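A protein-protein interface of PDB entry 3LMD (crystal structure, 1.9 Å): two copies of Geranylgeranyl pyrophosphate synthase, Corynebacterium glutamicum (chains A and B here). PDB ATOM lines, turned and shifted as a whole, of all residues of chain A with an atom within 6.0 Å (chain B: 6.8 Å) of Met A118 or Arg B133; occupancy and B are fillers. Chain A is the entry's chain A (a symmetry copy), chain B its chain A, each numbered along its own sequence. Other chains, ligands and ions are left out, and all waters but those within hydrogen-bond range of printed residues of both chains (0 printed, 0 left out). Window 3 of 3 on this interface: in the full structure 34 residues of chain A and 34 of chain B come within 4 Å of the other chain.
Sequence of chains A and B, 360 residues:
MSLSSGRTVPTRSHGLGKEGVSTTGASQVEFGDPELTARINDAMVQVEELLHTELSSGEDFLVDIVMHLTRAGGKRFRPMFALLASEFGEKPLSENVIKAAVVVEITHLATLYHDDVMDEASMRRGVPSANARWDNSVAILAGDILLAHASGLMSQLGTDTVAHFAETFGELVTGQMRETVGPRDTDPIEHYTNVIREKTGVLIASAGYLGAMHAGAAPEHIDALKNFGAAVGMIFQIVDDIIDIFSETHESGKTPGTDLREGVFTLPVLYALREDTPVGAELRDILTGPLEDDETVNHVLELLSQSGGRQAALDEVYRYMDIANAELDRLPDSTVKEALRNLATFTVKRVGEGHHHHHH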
ATOM      1  N   TYR A 113      -1.529  -5.906  17.654  1.00  0.00           N
ATOM      2  CA  TYR A 113      -1.254  -5.223  18.909  1.00  0.00           C
ATOM      3  C   TYR A 113      -2.188  -4.038  19.095  1.00  0.00           C
ATOM      4  O   TYR A 113      -2.699  -3.817  20.202  1.00  0.00           O
ATOM      5  CB  TYR A 113       0.215  -4.827  18.996  1.00  0.00           C
ATOM      6  CG  TYR A 113       1.100  -6.048  18.882  1.00  0.00           C
ATOM      7  CD1 TYR A 113       0.536  -7.329  18.921  1.00  0.00           C
ATOM      8  CD2 TYR A 113       2.473  -5.942  18.734  1.00  0.00           C
ATOM      9  CE1 TYR A 113       1.318  -8.480  18.815  1.00  0.00           C
ATOM     10  CE2 TYR A 113       3.277  -7.094  18.635  1.00  0.00           C
ATOM     11  CZ  TYR A 113       2.687  -8.358  18.681  1.00  0.00           C
ATOM     12  OH  TYR A 113       3.448  -9.509  18.580  1.00  0.00           O
ATOM     13  N   HIS A 114      -2.472  -3.289  18.027  1.00  0.00           N
ATOM     14  CA  HIS A 114      -3.412  -2.162  18.160  1.00  0.00           C
ATOM     15  C   HIS A 114      -4.857  -2.641  18.276  1.00  0.00           C
ATOM     16  O   HIS A 114      -5.668  -2.043  18.976  1.00  0.00           O
ATOM     17  CB  HIS A 114      -3.284  -1.184  16.994  1.00  0.00           C
ATOM     18  CG  HIS A 114      -2.056  -0.327  17.057  1.00  0.00           C
ATOM     19  ND1 HIS A 114      -1.054  -0.521  17.989  1.00  0.00           N
ATOM     20  CD2 HIS A 114      -1.666   0.725  16.300  1.00  0.00           C
ATOM     21  CE1 HIS A 114      -0.103   0.381  17.802  1.00  0.00           C
ATOM     22  NE2 HIS A 114      -0.452   1.149  16.785  1.00  0.00           N
ATOM     23  N   ASP A 115      -5.186  -3.708  17.565  1.00  0.00           N
ATOM     24  CA  ASP A 115      -6.510  -4.330  17.702  1.00  0.00           C
ATOM     25  C   ASP A 115      -6.788  -4.804  19.105  1.00  0.00           C
ATOM     26  O   ASP A 115      -7.872  -4.573  19.626  1.00  0.00           O
ATOM     27  CB  ASP A 115      -6.639  -5.545  16.794  1.00  0.00           C
ATOM     28  CG  ASP A 115      -7.331  -5.228  15.523  1.00  0.00           C
ATOM     29  OD1 ASP A 115      -7.922  -4.132  15.445  1.00  0.00           O
ATOM     30  OD2 ASP A 115      -7.298  -6.077  14.602  1.00  0.00           O
ATOM     31  N   ASP A 116      -5.843  -5.534  19.686  1.00  0.00           N
ATOM     32  CA  ASP A 116      -6.022  -6.105  21.021  1.00  0.00           C
ATOM     33  C   ASP A 116      -6.291  -5.027  22.081  1.00  0.00           C
ATOM     34  O   ASP A 116      -7.083  -5.234  23.001  1.00  0.00           O
ATOM     35  CB  ASP A 116      -4.827  -6.978  21.421  1.00  0.00           C
ATOM     36  CG  ASP A 116      -4.694  -8.250  20.560  1.00  0.00           C
ATOM     37  OD1 ASP A 116      -5.523  -8.484  19.640  1.00  0.00           O
ATOM     38  OD2 ASP A 116      -3.742  -9.022  20.810  1.00  0.00           O
ATOM     39  N   VAL A 117      -5.650  -3.872  21.950  1.00  0.00           N
ATOM     40  CA  VAL A 117      -5.879  -2.776  22.896  1.00  0.00           C
ATOM     41  C   VAL A 117      -7.316  -2.240  22.832  1.00  0.00           C
ATOM     42  O   VAL A 117      -7.885  -1.813  23.835  1.00  0.00           O
ATOM     43  CB  VAL A 117      -4.877  -1.625  22.687  1.00  0.00           C
ATOM     44  CG1 VAL A 117      -5.361  -0.357  23.378  1.00  0.00           C
ATOM     45  CG2 VAL A 117      -3.520  -2.023  23.212  1.00  0.00           C
ATOM     46  N   MET A 118      -7.911  -2.287  21.650  1.00  0.00           N
ATOM     47  CA  MET A 118      -9.289  -1.848  21.480  1.00  0.00           C
ATOM     48  C   MET A 118     -10.352  -2.903  21.830  1.00  0.00           C
ATOM     49  O   MET A 118     -11.336  -2.594  22.497  1.00  0.00           O
ATOM     50  CB  MET A 118      -9.458  -1.304  20.071  1.00  0.00           C
ATOM     51  CG  MET A 118      -8.383  -0.280  19.809  1.00  0.00           C
ATOM     52  SD  MET A 118      -8.513   0.552  18.238  1.00  0.00           S
ATOM     53  CE  MET A 118      -8.597  -0.842  17.130  1.00  0.00           C
ATOM     54  N   ASP A 119     -10.142  -4.140  21.391  1.00  0.00           N
ATOM     55  CA  ASP A 119     -11.049  -5.242  21.714  1.00  0.00           C
ATOM     56  C   ASP A 119     -11.071  -5.526  23.217  1.00  0.00           C
ATOM     57  O   ASP A 119     -10.899  -4.621  24.034  1.00  0.00           O
ATOM     58  CB  ASP A 119     -10.651  -6.509  20.951  1.00  0.00           C
ATOM     59  CG  ASP A 119     -10.728  -6.334  19.439  1.00  0.00           C
ATOM     60  OD1 ASP A 119     -11.246  -5.291  18.979  1.00  0.00           O
ATOM     61  OD2 ASP A 119     -10.267  -7.239  18.708  1.00  0.00           O
ATOM     62  N   GLN A 176     -10.417  -1.411  10.599  1.00  0.00           N
ATOM     63  CA  GLN A 176     -10.537  -1.367  12.070  1.00  0.00           C
ATOM     64  C   GLN A 176     -11.472  -0.224  12.518  1.00  0.00           C
ATOM     65  O   GLN A 176     -12.297  -0.389  13.417  1.00  0.00           O
ATOM     66  CB  GLN A 176      -9.144  -1.177  12.721  1.00  0.00           C
ATOM     67  CG  GLN A 176      -8.144  -2.305  12.404  1.00  0.00           C
ATOM     68  CD  GLN A 176      -6.706  -2.011  12.911  1.00  0.00           C
ATOM     69  OE1 GLN A 176      -5.946  -1.263  12.291  1.00  0.00           O
ATOM     70  NE2 GLN A 176      -6.341  -2.613  14.032  1.00  0.00           N
ATOM     71  N   THR A 180     -15.088  -0.459  14.370  1.00  0.00           N
ATOM     72  CA  THR A 180     -15.280   0.320  15.602  1.00  0.00           C
ATOM     73  C   THR A 180     -16.522   1.222  15.566  1.00  0.00           C
ATOM     74  O   THR A 180     -17.291   1.239  16.523  1.00  0.00           O
ATOM     75  CB  THR A 180     -14.035   1.175  15.958  1.00  0.00           C
ATOM     76  OG1 THR A 180     -12.923   0.305  16.163  1.00  0.00           O
ATOM     77  CG2 THR A 180     -14.271   1.958  17.256  1.00  0.00           C
ATOM     78  N   ASN B 131     -18.132   6.693  26.278  1.00  0.00           N
ATOM     79  CA  ASN B 131     -17.197   6.689  27.397  1.00  0.00           C
ATOM     80  C   ASN B 131     -15.748   6.906  26.951  1.00  0.00           C
ATOM     81  O   ASN B 131     -15.488   7.589  25.960  1.00  0.00           O
ATOM     82  CB  ASN B 131     -17.319   5.387  28.194  1.00  0.00           C
ATOM     83  CG  ASN B 131     -16.877   4.174  27.398  1.00  0.00           C
ATOM     84  OD1 ASN B 131     -16.887   4.188  26.164  1.00  0.00           O
ATOM     85  ND2 ASN B 131     -16.482   3.117  28.102  1.00  0.00           N
ATOM     86  N   ALA B 132     -14.812   6.315  27.688  1.00  0.00           N
ATOM     87  CA  ALA B 132     -13.388   6.511  27.425  1.00  0.00           C
ATOM     88  C   ALA B 132     -12.771   5.384  26.592  1.00  0.00           C
ATOM     89  O   ALA B 132     -11.728   5.569  25.966  1.00  0.00           O
ATOM     90  CB  ALA B 132     -12.624   6.690  28.740  1.00  0.00           C
ATOM     91  N   ARG B 133     -13.410   4.218  26.590  1.00  0.00           N
ATOM     92  CA  ARG B 133     -12.912   3.093  25.801  1.00  0.00           C
ATOM     93  C   ARG B 133     -12.940   3.428  24.306  1.00  0.00           C
ATOM     94  O   ARG B 133     -12.094   2.962  23.539  1.00  0.00           O
ATOM     95  CB  ARG B 133     -13.726   1.820  26.068  1.00  0.00           C
ATOM     96  CG  ARG B 133     -13.857   1.422  27.539  1.00  0.00           C
ATOM     97  CD  ARG B 133     -13.913  -0.103  27.697  1.00  0.00           C
ATOM     98  NE  ARG B 133     -14.564  -0.766  26.565  1.00  0.00           N
ATOM     99  CZ  ARG B 133     -13.924  -1.232  25.492  1.00  0.00           C
ATOM    100  NH1 ARG B 133     -12.607  -1.114  25.389  1.00  0.00           N
ATOM    101  NH2 ARG B 133     -14.603  -1.820  24.515  1.00  0.00           N
ATOM    102  N   TRP B 134     -13.913   4.244  23.904  1.00  0.00           N
ATOM    103  CA  TRP B 134     -14.069   4.628  22.503  1.00  0.00           C
ATOM    104  C   TRP B 134     -13.030   5.661  22.062  1.00  0.00           C
ATOM    105  O   TRP B 134     -12.404   5.509  21.009  1.00  0.00           O
ATOM    106  CB  TRP B 134     -15.479   5.164  22.243  1.00  0.00           C
ATOM    107  CG  TRP B 134     -15.880   5.140  20.792  1.00  0.00           C
ATOM    108  CD1 TRP B 134     -16.279   4.046  20.056  1.00  0.00           C
ATOM    109  CD2 TRP B 134     -15.925   6.261  19.899  1.00  0.00           C
ATOM    110  NE1 TRP B 134     -16.571   4.429  18.765  1.00  0.00           N
ATOM    111  CE2 TRP B 134     -16.361   5.778  18.643  1.00  0.00           C
ATOM    112  CE3 TRP B 134     -15.635   7.621  20.037  1.00  0.00           C
ATOM    113  CZ2 TRP B 134     -16.517   6.612  17.539  1.00  0.00           C
ATOM    114  CZ3 TRP B 134     -15.791   8.444  18.941  1.00  0.00           C
ATOM    115  CH2 TRP B 134     -16.228   7.940  17.708  1.00  0.00           C
ATOM    116  N   ASP B 135     -12.856   6.706  22.866  1.00  0.00           N
ATOM    117  CA  ASP B 135     -11.892   7.763  22.565  1.00  0.00           C
ATOM    118  C   ASP B 135     -10.473   7.212  22.392  1.00  0.00           C
ATOM    119  O   ASP B 135      -9.685   7.701  21.572  1.00  0.00           O
ATOM    120  CB  ASP B 135     -11.908   8.820  23.671  1.00  0.00           C
ATOM    121  CG  ASP B 135     -13.242   9.558  23.756  1.00  0.00           C
ATOM    122  OD1 ASP B 135     -14.064   9.423  22.820  1.00  0.00           O
ATOM    123  OD2 ASP B 135     -13.461  10.273  24.758  1.00  0.00           O
ATOM    124  N   ASN B 136     -10.143   6.191  23.168  1.00  0.00           N
ATOM    125  CA  ASN B 136      -8.818   5.621  23.077  1.00  0.00           C
ATOM    126  C   ASN B 136      -8.670   4.819  21.792  1.00  0.00           C
ATOM    127  O   ASN B 136      -7.690   4.958  21.056  1.00  0.00           O
ATOM    128  CB  ASN B 136      -8.515   4.770  24.308  1.00  0.00           C
ATOM    129  CG  ASN B 136      -8.076   5.610  25.498  1.00  0.00           C
ATOM    130  OD1 ASN B 136      -8.035   6.841  25.430  1.00  0.00           O
ATOM    131  ND2 ASN B 136      -7.734   4.947  26.589  1.00  0.00           N
ATOM    132  N   SER B 137      -9.658   3.988  21.508  1.00  0.00           N
ATOM    133  CA  SER B 137      -9.621   3.258  20.271  1.00  0.00           C
ATOM    134  C   SER B 137      -9.464   4.239  19.125  1.00  0.00           C
ATOM    135  O   SER B 137      -8.624   4.040  18.253  1.00  0.00           O
ATOM    136  CB  SER B 137     -10.863   2.380  20.092  1.00  0.00           C
ATOM    137  OG  SER B 137     -10.674   1.153  20.781  1.00  0.00           O
ATOM    138  N   VAL B 138     -10.244   5.311  19.111  1.00  0.00           N
ATOM    139  CA  VAL B 138     -10.231   6.099  17.895  1.00  0.00           C
ATOM    140  C   VAL B 138      -8.959   6.920  17.775  1.00  0.00           C
ATOM    141  O   VAL B 138      -8.472   7.118  16.671  1.00  0.00           O
ATOM    142  CB  VAL B 138     -11.532   6.905  17.609  1.00  0.00           C
ATOM    143  CG1 VAL B 138     -12.756   6.005  17.733  1.00  0.00           C
ATOM    144  CG2 VAL B 138     -11.622   8.184  18.464  1.00  0.00           C
ATOM    145  N   ILE B 140      -6.007   5.928  18.732  1.00  0.00           N
ATOM    146  CA  ILE B 140      -4.976   4.995  18.272  1.00  0.00           C
ATOM    147  C   ILE B 140      -5.085   4.893  16.755  1.00  0.00           C
ATOM    148  O   ILE B 140      -4.080   4.924  16.038  1.00  0.00           O
ATOM    149  CB  ILE B 140      -5.204   3.628  18.854  1.00  0.00           C
ATOM    150  CG1 ILE B 140      -4.873   3.645  20.353  1.00  0.00           C
ATOM    151  CG2 ILE B 140      -4.268   2.577  18.170  1.00  0.00           C
ATOM    152  CD1 ILE B 140      -5.351   2.311  21.071  1.00  0.00           C
ATOM    153  N   LEU B 141      -6.320   4.751  16.273  1.00  0.00           N
ATOM    154  CA  LEU B 141      -6.545   4.579  14.850  1.00  0.00           C
ATOM    155  C   LEU B 141      -6.297   5.875  14.072  1.00  0.00           C
ATOM    156  O   LEU B 141      -5.817   5.836  12.928  1.00  0.00           O
ATOM    157  CB  LEU B 141      -7.946   4.023  14.555  1.00  0.00           C
ATOM    158  CG  LEU B 141      -8.155   2.590  15.097  1.00  0.00           C
ATOM    159  CD1 LEU B 141      -9.580   2.117  14.781  1.00  0.00           C
ATOM    160  CD2 LEU B 141      -7.138   1.632  14.525  1.00  0.00           C
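O of Met A118 lies within hydrogen-bond range of NH1 of Arg B133 (3.5 Å).
The side-chain sulfur (SD) of Met A118 lies close to the side-chain hydroxyl (OG) of Ser B137, at 3.4 Å.
OD1 of Asp A115 sits at hydrogen-bond distance from NE2 of Gln A176 (2.6 Å).
OG1 of Thr A180 lies within hydrogen-bond range of O of Gln A176 (2.9 Å).
His A114 touches Ile B140 (CD2 to CG2, 3.7 Å).
Val A117 touches Ile B140.
Leu B141 touches Met A118 (CG to SD, 3.8 Å).
CD1 of Leu B141 touches C of Gln A176 (3.8 Å).
Thr A180 touches Trp B134.
Arg B133 touches just one residue of chain A: Met A118.
Of the printed residues of chain B, His A114 touches Ile B140 (3.7 Å).
Of the printed residues of chain A, Leu B141 touches Met A118 and Gln A176.
Printed residues of chain B within 4 Å of Gln A176: Leu B141.
Asn B131 touches none of the printed residues of chain A.
The nearest residue of chain A that does not touch Arg B133 is Asp A119 (4.1 Å).
Of the 10 printed residues of chain B, 5 touch a printed residue of chain A.
Printed residues of chain B that touch a printed residue of chain A: Arg B133, Trp B134, Ser B137, Ile B140 and Leu B141.
Among the printed residues, no Asp or Glu carboxylate lies within 4 Å of a Lys or Arg side-chain nitrogen of the other chain.
No position is printed for both chains.
Of the 7 pairs that touch across the chains among the printed residues, none has its exchanged pair printed and touching as well.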
